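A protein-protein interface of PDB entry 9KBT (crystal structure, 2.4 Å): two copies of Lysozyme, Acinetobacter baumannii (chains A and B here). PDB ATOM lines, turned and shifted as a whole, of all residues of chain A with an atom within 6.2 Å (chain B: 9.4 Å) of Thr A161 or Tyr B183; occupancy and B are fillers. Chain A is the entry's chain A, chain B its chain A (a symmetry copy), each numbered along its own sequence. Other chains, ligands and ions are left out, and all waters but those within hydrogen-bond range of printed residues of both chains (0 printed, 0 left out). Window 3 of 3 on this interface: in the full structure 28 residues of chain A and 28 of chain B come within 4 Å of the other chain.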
ATOM      1  N   PHE A 157      31.307   3.127  -0.430  1.00  0.00           N
ATOM      2  CA  PHE A 157      31.359   2.806   0.992  1.00  0.00           C
ATOM      3  C   PHE A 157      30.261   3.520   1.765  1.00  0.00           C
ATOM      4  O   PHE A 157      29.716   2.961   2.726  1.00  0.00           O
ATOM      5  CB  PHE A 157      32.735   3.172   1.549  1.00  0.00           C
ATOM      6  CG  PHE A 157      32.988   2.683   2.952  1.00  0.00           C
ATOM      7  CD1 PHE A 157      32.847   1.338   3.273  1.00  0.00           C
ATOM      8  CD2 PHE A 157      33.386   3.571   3.945  1.00  0.00           C
ATOM      9  CE1 PHE A 157      33.089   0.888   4.569  1.00  0.00           C
ATOM     10  CE2 PHE A 157      33.626   3.138   5.233  1.00  0.00           C
ATOM     11  CZ  PHE A 157      33.478   1.789   5.553  1.00  0.00           C
ATOM     12  N   SER A 158      29.903   4.737   1.343  1.00  0.00           N
ATOM     13  CA  SER A 158      28.928   5.540   2.074  1.00  0.00           C
ATOM     14  C   SER A 158      27.492   5.065   1.883  1.00  0.00           C
ATOM     15  O   SER A 158      26.619   5.456   2.664  1.00  0.00           O
ATOM     16  CB  SER A 158      29.035   6.987   1.640  1.00  0.00           C
ATOM     17  OG  SER A 158      28.521   7.137   0.336  1.00  0.00           O
ATOM     18  N   LYS A 159      27.224   4.260   0.853  1.00  0.00           N
ATOM     19  CA  LYS A 159      25.898   3.712   0.587  1.00  0.00           C
ATOM     20  C   LYS A 159      25.805   2.231   0.940  1.00  0.00           C
ATOM     21  O   LYS A 159      24.787   1.591   0.648  1.00  0.00           O
ATOM     22  CB  LYS A 159      25.512   3.892  -0.888  1.00  0.00           C
ATOM     23  CG  LYS A 159      25.097   5.285  -1.370  1.00  0.00           C
ATOM     24  CD  LYS A 159      25.760   6.426  -0.651  1.00  0.00           C
ATOM     25  CE  LYS A 159      25.017   7.723  -0.876  1.00  0.00           C
ATOM     26  NZ  LYS A 159      25.582   8.819  -0.029  1.00  0.00           N
ATOM     27  N   SER A 160      26.848   1.666   1.536  1.00  0.00           N
ATOM     28  CA  SER A 160      26.928   0.222   1.683  1.00  0.00           C
ATOM     29  C   SER A 160      26.081  -0.258   2.856  1.00  0.00           C
ATOM     30  O   SER A 160      26.075   0.352   3.930  1.00  0.00           O
ATOM     31  CB  SER A 160      28.386  -0.198   1.875  1.00  0.00           C
ATOM     32  OG  SER A 160      28.972   0.525   2.942  1.00  0.00           O
ATOM     33  N   THR A 161      25.354  -1.357   2.647  1.00  0.00           N
ATOM     34  CA  THR A 161      24.818  -2.067   3.806  1.00  0.00           C
ATOM     35  C   THR A 161      25.949  -2.485   4.733  1.00  0.00           C
ATOM     36  O   THR A 161      25.756  -2.568   5.952  1.00  0.00           O
ATOM     37  CB  THR A 161      24.000  -3.298   3.390  1.00  0.00           C
ATOM     38  OG1 THR A 161      24.613  -3.953   2.273  1.00  0.00           O
ATOM     39  CG2 THR A 161      22.596  -2.902   3.001  1.00  0.00           C
ATOM     40  N   MET A 162      27.142  -2.719   4.170  1.00  0.00           N
ATOM     41  CA  MET A 162      28.306  -3.046   4.985  1.00  0.00           C
ATOM     42  C   MET A 162      28.629  -1.927   5.966  1.00  0.00           C
ATOM     43  O   MET A 162      29.041  -2.191   7.101  1.00  0.00           O
ATOM     44  CB  MET A 162      29.517  -3.344   4.096  1.00  0.00           C
ATOM     45  CG  MET A 162      30.718  -3.818   4.905  1.00  0.00           C
ATOM     46  SD  MET A 162      32.371  -3.722   4.183  1.00  0.00           S
ATOM     47  CE  MET A 162      33.112  -2.668   5.430  1.00  0.00           C
ATOM     48  N   LEU A 163      28.405  -0.677   5.606  1.00  0.00           N
ATOM     49  CA  LEU A 163      28.643   0.411   6.549  1.00  0.00           C
ATOM     50  C   LEU A 163      27.581   0.454   7.618  1.00  0.00           C
ATOM     51  O   LEU A 163      27.816   0.918   8.722  1.00  0.00           O
ATOM     52  CB  LEU A 163      28.728   1.766   5.842  1.00  0.00           C
ATOM     53  CG  LEU A 163      29.052   3.035   6.632  1.00  0.00           C
ATOM     54  CD1 LEU A 163      30.372   2.898   7.354  1.00  0.00           C
ATOM     55  CD2 LEU A 163      29.039   4.283   5.775  1.00  0.00           C
ATOM     56  N   LYS A 164      26.393  -0.022   7.294  1.00  0.00           N
ATOM     57  CA  LYS A 164      25.298   0.020   8.258  1.00  0.00           C
ATOM     58  C   LYS A 164      25.644  -0.803   9.469  1.00  0.00           C
ATOM     59  O   LYS A 164      25.503  -0.347  10.595  1.00  0.00           O
ATOM     60  CB  LYS A 164      23.997  -0.477   7.645  1.00  0.00           C
ATOM     61  N   SER A 165      26.146  -2.011   9.222  1.00  0.00           N
ATOM     62  CA  SER A 165      26.505  -2.916  10.305  1.00  0.00           C
ATOM     63  C   SER A 165      27.817  -2.529  10.967  1.00  0.00           C
ATOM     64  O   SER A 165      28.225  -3.136  11.942  1.00  0.00           O
ATOM     65  CB  SER A 165      26.603  -4.336   9.754  1.00  0.00           C
ATOM     66  OG  SER A 165      27.277  -4.345   8.507  1.00  0.00           O
ATOM     67  N   LEU A 166      28.493  -1.518  10.443  1.00  0.00           N
ATOM     68  CA  LEU A 166      29.715  -1.068  11.090  1.00  0.00           C
ATOM     69  C   LEU A 166      29.376  -0.167  12.253  1.00  0.00           C
ATOM     70  O   LEU A 166      29.807  -0.400  13.378  1.00  0.00           O
ATOM     71  CB  LEU A 166      30.597  -0.310  10.114  1.00  0.00           C
ATOM     72  CG  LEU A 166      31.964  -0.914   9.841  1.00  0.00           C
ATOM     73  CD1 LEU A 166      32.076  -2.326  10.389  1.00  0.00           C
ATOM     74  CD2 LEU A 166      32.174  -0.900   8.346  1.00  0.00           C
ATOM     75  N   GLN A 177      29.669  -9.176   4.536  1.00  0.00           N
ATOM     76  CA  GLN A 177      29.294  -8.279   3.447  1.00  0.00           C
ATOM     77  C   GLN A 177      30.377  -8.216   2.377  1.00  0.00           C
ATOM     78  O   GLN A 177      30.062  -8.075   1.189  1.00  0.00           O
ATOM     79  CB  GLN A 177      28.996  -6.880   3.986  1.00  0.00           C
ATOM     80  CG  GLN A 177      27.513  -6.570   4.191  1.00  0.00           C
ATOM     81  CD  GLN A 177      26.614  -7.042   3.049  1.00  0.00           C
ATOM     82  OE1 GLN A 177      26.783  -6.645   1.892  1.00  0.00           O
ATOM     83  NE2 GLN A 177      25.648  -7.895   3.378  1.00  0.00           N
ATOM     84  N   TRP A 181      30.350  -8.240  -2.617  1.00  0.00           N
ATOM     85  CA  TRP A 181      30.959  -7.373  -3.610  1.00  0.00           C
ATOM     86  C   TRP A 181      31.872  -8.095  -4.548  1.00  0.00           C
ATOM     87  O   TRP A 181      33.049  -7.839  -4.566  1.00  0.00           O
ATOM     88  CB  TRP A 181      31.765  -6.303  -2.904  1.00  0.00           C
ATOM     89  CG  TRP A 181      30.979  -5.419  -1.994  1.00  0.00           C
ATOM     90  CD1 TRP A 181      30.626  -5.676  -0.709  1.00  0.00           C
ATOM     91  CD2 TRP A 181      30.474  -4.117  -2.294  1.00  0.00           C
ATOM     92  NE1 TRP A 181      29.922  -4.625  -0.189  1.00  0.00           N
ATOM     93  CE2 TRP A 181      29.816  -3.651  -1.143  1.00  0.00           C
ATOM     94  CE3 TRP A 181      30.507  -3.301  -3.425  1.00  0.00           C
ATOM     95  CZ2 TRP A 181      29.201  -2.409  -1.090  1.00  0.00           C
ATOM     96  CZ3 TRP A 181      29.894  -2.068  -3.368  1.00  0.00           C
ATOM     97  CH2 TRP A 181      29.253  -1.633  -2.212  1.00  0.00           C
ATOM     98  N   GLY B  21      26.734  10.520  -5.309  1.00  0.00           N
ATOM     99  CA  GLY B  21      25.986  10.078  -4.150  1.00  0.00           C
ATOM    100  C   GLY B  21      24.674  10.777  -3.890  1.00  0.00           C
ATOM    101  O   GLY B  21      24.200  10.757  -2.755  1.00  0.00           O
ATOM    102  N   ASN B 151      18.651   7.482  -9.964  1.00  0.00           N
ATOM    103  CA  ASN B 151      18.924   7.828  -8.577  1.00  0.00           C
ATOM    104  C   ASN B 151      20.302   7.350  -8.139  1.00  0.00           C
ATOM    105  O   ASN B 151      20.988   8.043  -7.379  1.00  0.00           O
ATOM    106  CB  ASN B 151      17.859   7.243  -7.656  1.00  0.00           C
ATOM    107  CG  ASN B 151      18.143   7.540  -6.199  1.00  0.00           C
ATOM    108  OD1 ASN B 151      18.250   6.632  -5.372  1.00  0.00           O
ATOM    109  ND2 ASN B 151      18.305   8.822  -5.883  1.00  0.00           N
ATOM    110  N   VAL B 152      20.726   6.176  -8.602  1.00  0.00           N
ATOM    111  CA  VAL B 152      21.832   5.482  -7.975  1.00  0.00           C
ATOM    112  C   VAL B 152      23.109   5.547  -8.801  1.00  0.00           C
ATOM    113  O   VAL B 152      24.203   5.462  -8.227  1.00  0.00           O
ATOM    114  CB  VAL B 152      21.444   4.018  -7.660  1.00  0.00           C
ATOM    115  CG1 VAL B 152      21.517   3.133  -8.901  1.00  0.00           C
ATOM    116  CG2 VAL B 152      22.307   3.475  -6.551  1.00  0.00           C
ATOM    117  N   THR B 161      24.663  -6.429  -6.967  1.00  0.00           N
ATOM    118  CA  THR B 161      24.087  -7.771  -6.963  1.00  0.00           C
ATOM    119  C   THR B 161      22.733  -7.762  -7.658  1.00  0.00           C
ATOM    120  O   THR B 161      22.337  -8.767  -8.261  1.00  0.00           O
ATOM    121  CB  THR B 161      23.938  -8.323  -5.537  1.00  0.00           C
ATOM    122  OG1 THR B 161      23.534  -7.283  -4.638  1.00  0.00           O
ATOM    123  CG2 THR B 161      25.246  -8.897  -5.047  1.00  0.00           C
ATOM    124  N   GLN B 177      15.951  -6.725  -4.259  1.00  0.00           N
ATOM    125  CA  GLN B 177      17.206  -5.998  -4.089  1.00  0.00           C
ATOM    126  C   GLN B 177      16.965  -4.505  -3.900  1.00  0.00           C
ATOM    127  O   GLN B 177      17.712  -3.849  -3.164  1.00  0.00           O
ATOM    128  CB  GLN B 177      18.129  -6.242  -5.283  1.00  0.00           C
ATOM    129  CG  GLN B 177      19.203  -7.307  -5.060  1.00  0.00           C
ATOM    130  CD  GLN B 177      19.892  -7.222  -3.698  1.00  0.00           C
ATOM    131  OE1 GLN B 177      20.491  -6.202  -3.344  1.00  0.00           O
ATOM    132  NE2 GLN B 177      19.810  -8.305  -2.931  1.00  0.00           N
ATOM    133  N   PHE B 178      15.935  -3.953  -4.558  1.00  0.00           N
ATOM    134  CA  PHE B 178      15.554  -2.554  -4.388  1.00  0.00           C
ATOM    135  C   PHE B 178      15.541  -2.174  -2.915  1.00  0.00           C
ATOM    136  O   PHE B 178      16.026  -1.103  -2.535  1.00  0.00           O
ATOM    137  CB  PHE B 178      14.170  -2.271  -4.984  1.00  0.00           C
ATOM    138  CG  PHE B 178      14.126  -2.282  -6.485  1.00  0.00           C
ATOM    139  CD1 PHE B 178      14.094  -3.476  -7.186  1.00  0.00           C
ATOM    140  CD2 PHE B 178      14.091  -1.090  -7.197  1.00  0.00           C
ATOM    141  CE1 PHE B 178      14.042  -3.487  -8.569  1.00  0.00           C
ATOM    142  CE2 PHE B 178      14.036  -1.090  -8.583  1.00  0.00           C
ATOM    143  CZ  PHE B 178      14.013  -2.292  -9.270  1.00  0.00           C
ATOM    144  N   ASP B 179      15.013  -3.068  -2.077  1.00  0.00           N
ATOM    145  CA  ASP B 179      14.837  -2.762  -0.661  1.00  0.00           C
ATOM    146  C   ASP B 179      16.173  -2.489   0.036  1.00  0.00           C
ATOM    147  O   ASP B 179      16.270  -1.579   0.870  1.00  0.00           O
ATOM    148  CB  ASP B 179      14.090  -3.916   0.010  1.00  0.00           C
ATOM    149  CG  ASP B 179      12.714  -4.168  -0.614  1.00  0.00           C
ATOM    150  OD1 ASP B 179      12.265  -3.347  -1.453  1.00  0.00           O
ATOM    151  OD2 ASP B 179      12.096  -5.204  -0.274  1.00  0.00           O
ATOM    152  N   LYS B 180      17.200  -3.266  -0.282  1.00  0.00           N
ATOM    153  CA  LYS B 180      18.504  -3.105   0.382  1.00  0.00           C
ATOM    154  C   LYS B 180      19.148  -1.721   0.229  1.00  0.00           C
ATOM    155  O   LYS B 180      19.880  -1.282   1.106  1.00  0.00           O
ATOM    156  CB  LYS B 180      19.449  -4.189  -0.082  1.00  0.00           C
ATOM    157  N   TRP B 181      18.865  -1.024  -0.865  1.00  0.00           N
ATOM    158  CA  TRP B 181      19.437   0.289  -1.106  1.00  0.00           C
ATOM    159  C   TRP B 181      18.728   1.387  -0.382  1.00  0.00           C
ATOM    160  O   TRP B 181      18.158   2.251  -0.998  1.00  0.00           O
ATOM    161  CB  TRP B 181      19.374   0.589  -2.589  1.00  0.00           C
ATOM    162  CG  TRP B 181      20.121  -0.365  -3.459  1.00  0.00           C
ATOM    163  CD1 TRP B 181      19.685  -1.566  -3.918  1.00  0.00           C
ATOM    164  CD2 TRP B 181      21.431  -0.184  -4.000  1.00  0.00           C
ATOM    165  NE1 TRP B 181      20.641  -2.152  -4.702  1.00  0.00           N
ATOM    166  CE2 TRP B 181      21.725  -1.321  -4.770  1.00  0.00           C
ATOM    167  CE3 TRP B 181      22.388   0.828  -3.904  1.00  0.00           C
ATOM    168  CZ2 TRP B 181      22.930  -1.474  -5.440  1.00  0.00           C
ATOM    169  CZ3 TRP B 181      23.584   0.670  -4.570  1.00  0.00           C
ATOM    170  CH2 TRP B 181      23.844  -0.468  -5.328  1.00  0.00           C
ATOM    171  N   VAL B 182      18.808   1.406   0.924  1.00  0.00           N
ATOM    172  CA  VAL B 182      18.056   2.373   1.688  1.00  0.00           C
ATOM    173  C   VAL B 182      19.019   3.072   2.608  1.00  0.00           C
ATOM    174  O   VAL B 182      18.730   4.078   3.244  1.00  0.00           O
ATOM    175  CB  VAL B 182      16.912   1.664   2.447  1.00  0.00           C
ATOM    176  CG1 VAL B 182      17.413   0.478   3.232  1.00  0.00           C
ATOM    177  CG2 VAL B 182      16.159   2.584   3.353  1.00  0.00           C
ATOM    178  N   TYR B 183      20.227   2.559   2.632  1.00  0.00           N
ATOM    179  CA  TYR B 183      21.178   3.149   3.540  1.00  0.00           C
ATOM    180  C   TYR B 183      21.977   4.220   2.830  1.00  0.00           C
ATOM    181  O   TYR B 183      22.286   4.109   1.641  1.00  0.00           O
ATOM    182  CB  TYR B 183      22.091   2.075   4.133  1.00  0.00           C
ATOM    183  CG  TYR B 183      21.306   0.967   4.796  1.00  0.00           C
ATOM    184  CD1 TYR B 183      20.965   1.041   6.142  1.00  0.00           C
ATOM    185  CD2 TYR B 183      20.888  -0.142   4.075  1.00  0.00           C
ATOM    186  CE1 TYR B 183      20.240   0.029   6.759  1.00  0.00           C
ATOM    187  CE2 TYR B 183      20.162  -1.160   4.682  1.00  0.00           C
ATOM    188  CZ  TYR B 183      19.841  -1.073   6.025  1.00  0.00           C
ATOM    189  OH  TYR B 183      19.120  -2.089   6.627  1.00  0.00           O
ATOM    190  N   ASP B 184      22.256   5.279   3.570  1.00  0.00           N
ATOM    191  CA  ASP B 184      23.152   6.338   3.162  1.00  0.00           C
ATOM    192  C   ASP B 184      23.921   6.740   4.404  1.00  0.00           C
ATOM    193  O   ASP B 184      23.308   6.992   5.446  1.00  0.00           O
ATOM    194  CB  ASP B 184      22.384   7.536   2.603  1.00  0.00           C
ATOM    195  CG  ASP B 184      23.302   8.670   2.167  1.00  0.00           C
ATOM    196  OD1 ASP B 184      24.093   9.183   2.988  1.00  0.00           O
ATOM    197  OD2 ASP B 184      23.202   9.073   0.993  1.00  0.00           O
ATOM    198  N   ASN B 185      25.251   6.798   4.296  1.00  0.00           N
ATOM    199  CA  ASN B 185      26.095   7.208   5.414  1.00  0.00           C
ATOM    200  C   ASN B 185      25.899   6.267   6.602  1.00  0.00           C
ATOM    201  O   ASN B 185      25.826   6.692   7.756  1.00  0.00           O
ATOM    202  CB  ASN B 185      25.808   8.665   5.789  1.00  0.00           C
ATOM    203  CG  ASN B 185      26.822   9.241   6.751  1.00  0.00           C
ATOM    204  OD1 ASN B 185      27.859   8.637   7.015  1.00  0.00           O
ATOM    205  ND2 ASN B 185      26.537  10.434   7.267  1.00  0.00           N
ATOM    206  N   GLY B 186      25.785   4.970   6.314  1.00  0.00           N
ATOM    207  CA  GLY B 186      25.517   3.986   7.347  1.00  0.00           C
ATOM    208  C   GLY B 186      24.109   4.013   7.920  1.00  0.00           C
ATOM    209  O   GLY B 186      23.693   3.056   8.582  1.00  0.00           O
ATOM    210  N   LYS B 187      23.365   5.091   7.669  1.00  0.00           N
ATOM    211  CA  LYS B 187      22.035   5.299   8.227  1.00  0.00           C
ATOM    212  C   LYS B 187      20.955   4.796   7.282  1.00  0.00           C
ATOM    213  O   LYS B 187      21.162   4.662   6.077  1.00  0.00           O
ATOM    214  CB  LYS B 187      21.782   6.776   8.516  1.00  0.00           C
ATOM    215  CG  LYS B 187      22.278   7.243   9.869  1.00  0.00           C
ATOM    216  CD  LYS B 187      22.074   8.739  10.029  1.00  0.00           C
ATOM    217  CE  LYS B 187      20.760   9.189   9.383  1.00  0.00           C
ATOM    218  NZ  LYS B 187      19.952  10.086  10.264  1.00  0.00           N
ATOM    219  N   LEU B 188      19.782   4.532   7.850  1.00  0.00           N
ATOM    220  CA  LEU B 188      18.605   4.184   7.069  1.00  0.00           C
ATOM    221  C   LEU B 188      17.804   5.443   6.781  1.00  0.00           C
ATOM    222  O   LEU B 188      17.587   6.274   7.669  1.00  0.00           O
ATOM    223  CB  LEU B 188      17.743   3.167   7.817  1.00  0.00           C
ATOM    224  CG  LEU B 188      16.663   2.416   7.038  1.00  0.00           C
ATOM    225  CD1 LEU B 188      16.314   1.159   7.794  1.00  0.00           C
ATOM    226  CD2 LEU B 188      15.411   3.260   6.821  1.00  0.00           C
ATOM    227  N   ILE B 189      17.369   5.586   5.532  1.00  0.00           N
ATOM    228  CA  ILE B 189      16.710   6.803   5.069  1.00  0.00           C
ATOM    229  C   ILE B 189      15.275   6.455   4.706  1.00  0.00           C
ATOM    230  O   ILE B 189      15.035   5.573   3.869  1.00  0.00           O
ATOM    231  CB  ILE B 189      17.462   7.443   3.891  1.00  0.00           C
ATOM    232  CG1 ILE B 189      18.966   7.401   4.151  1.00  0.00           C
ATOM    233  CG2 ILE B 189      17.031   8.874   3.695  1.00  0.00           C
ATOM    234  CD1 ILE B 189      19.374   8.092   5.425  1.00  0.00           C
ATOM    235  N   LYS B 190      14.322   7.138   5.352  1.00  0.00           N
ATOM    236  CA  LYS B 190      12.910   6.818   5.156  1.00  0.00           C
ATOM    237  C   LYS B 190      12.483   7.076   3.718  1.00  0.00           C
ATOM    238  O   LYS B 190      11.742   6.277   3.130  1.00  0.00           O
ATOM    239  CB  LYS B 190      12.049   7.629   6.126  1.00  0.00           C
ATOM    240  N   GLY B 191      12.957   8.187   3.134  1.00  0.00           N
ATOM    241  CA  GLY B 191      12.664   8.464   1.738  1.00  0.00           C
ATOM    242  C   GLY B 191      13.141   7.358   0.821  1.00  0.00           C
ATOM    243  O   GLY B 191      12.459   6.996  -0.141  1.00  0.00           O
ATOM    244  N   LEU B 192      14.298   6.775   1.130  1.00  0.00           N
ATOM    245  CA  LEU B 192      14.856   5.750   0.259  1.00  0.00           C
ATOM    246  C   LEU B 192      13.991   4.496   0.260  1.00  0.00           C
ATOM    247  O   LEU B 192      13.549   4.043  -0.800  1.00  0.00           O
ATOM    248  CB  LEU B 192      16.295   5.437   0.671  1.00  0.00           C
ATOM    249  CG  LEU B 192      17.317   6.527   0.333  1.00  0.00           C
ATOM    250  CD1 LEU B 192      18.723   6.108   0.717  1.00  0.00           C
ATOM    251  CD2 LEU B 192      17.238   6.868  -1.141  1.00  0.00           C
ATOM    252  N   VAL B 193      13.720   3.928   1.438  1.00  0.00           N
ATOM    253  CA  VAL B 193      12.826   2.772   1.482  1.00  0.00           C
ATOM    254  C   VAL B 193      11.460   3.150   0.944  1.00  0.00           C
ATOM    255  O   VAL B 193      10.837   2.375   0.207  1.00  0.00           O
ATOM    256  CB  VAL B 193      12.728   2.182   2.902  1.00  0.00           C
ATOM    257  CG1 VAL B 193      12.419   3.269   3.920  1.00  0.00           C
ATOM    258  CG2 VAL B 193      11.689   1.057   2.939  1.00  0.00           C
ATOM    259  N   ARG B 196      12.473   3.184  -2.664  1.00  0.00           N
ATOM    260  CA  ARG B 196      12.711   1.779  -2.991  1.00  0.00           C
ATOM    261  C   ARG B 196      11.408   0.994  -3.074  1.00  0.00           C
ATOM    262  O   ARG B 196      11.198   0.205  -4.007  1.00  0.00           O
ATOM    263  CB  ARG B 196      13.621   1.142  -1.942  1.00  0.00           C
ATOM    264  CG  ARG B 196      15.008   1.695  -1.869  1.00  0.00           C
ATOM    265  CD  ARG B 196      15.628   1.829  -3.230  1.00  0.00           C
ATOM    266  NE  ARG B 196      16.612   2.901  -3.208  1.00  0.00           N
ATOM    267  CZ  ARG B 196      16.873   3.704  -4.228  1.00  0.00           C
ATOM    268  NH1 ARG B 196      16.253   3.568  -5.389  1.00  0.00           N
ATOM    269  NH2 ARG B 196      17.778   4.663  -4.080  1.00  0.00           N
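OD2 of Asp B184 is in salt-bridge range of NZ of Lys A159, at 2.6 Å. The backbone carbonyl oxygen (O) of Ser A158 lies within hydrogen-bond range of the backbone NH (N) of Asn B185, 2.5 Å away.
The side-chain hydroxyl of Ser A160 lies within hydrogen-bond range of the backbone NH of Leu A163 (3.0 Å). The backbone carbonyl oxygen (O) of Thr A161 is in hydrogen-bond range of the side-chain hydroxyl (OG) of Ser A165 (3.5 Å). The side-chain hydroxyl (OG1) of Thr A161 sits at hydrogen-bond distance from the side-chain amide oxygen (OE1) of Gln A177 (3.5 Å). The side-chain hydroxyl of Ser A158 lies close to the side-chain amino group of Lys A159, at 3.4 Å.
Among the printed residues, merely in contact across the chains: Leu A163 with Gly B186 (3.4 Å), Thr A161 with Tyr B183 (3.4 Å), Lys A164 with Gly B186 (3.4 Å), Ser A158 with Asp B184 (3.5 Å), Lys A159 with Gly B21 (3.6 Å), Lys A159 with Tyr B183 (3.7 Å), Thr A161 with Lys B180 (3.7 Å), Lys A164 with Tyr B183 (3.7 Å), Ser A158 with Gly B186 (3.8 Å) and Leu A163 with Asn B185 (3.8 Å).
Of chain B, only Lys B180 and Tyr B183 come within 4 Å of Thr A161. Tyr B183 touches three residues of chain A. Of chain B, only Tyr B183 and Gly B186 come within 4 Å of Lys A164. Printed residues of chain A within 4 Å of Asp B184: Ser A158 and Lys A159. Of the printed residues of chain B, Leu A163 touches Asn B185 and Gly B186. Gln A177 touches none of the printed residues of chain B. Trp A181 touches none of the printed residues of chain B.
Hydrophobic or aromatic side chains of chain A within 4 Å of the printed part of chain B: Leu A163. Printed residues of chain B that touch a printed residue of chain A: Gly B21, Lys B180, Tyr B183, Asp B184, Asn B185 and Gly B186.
3 positions are printed for both chains. Of the 12 pairs that touch across the chains among the printed residues, none has its exchanged pair printed and touching as well.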
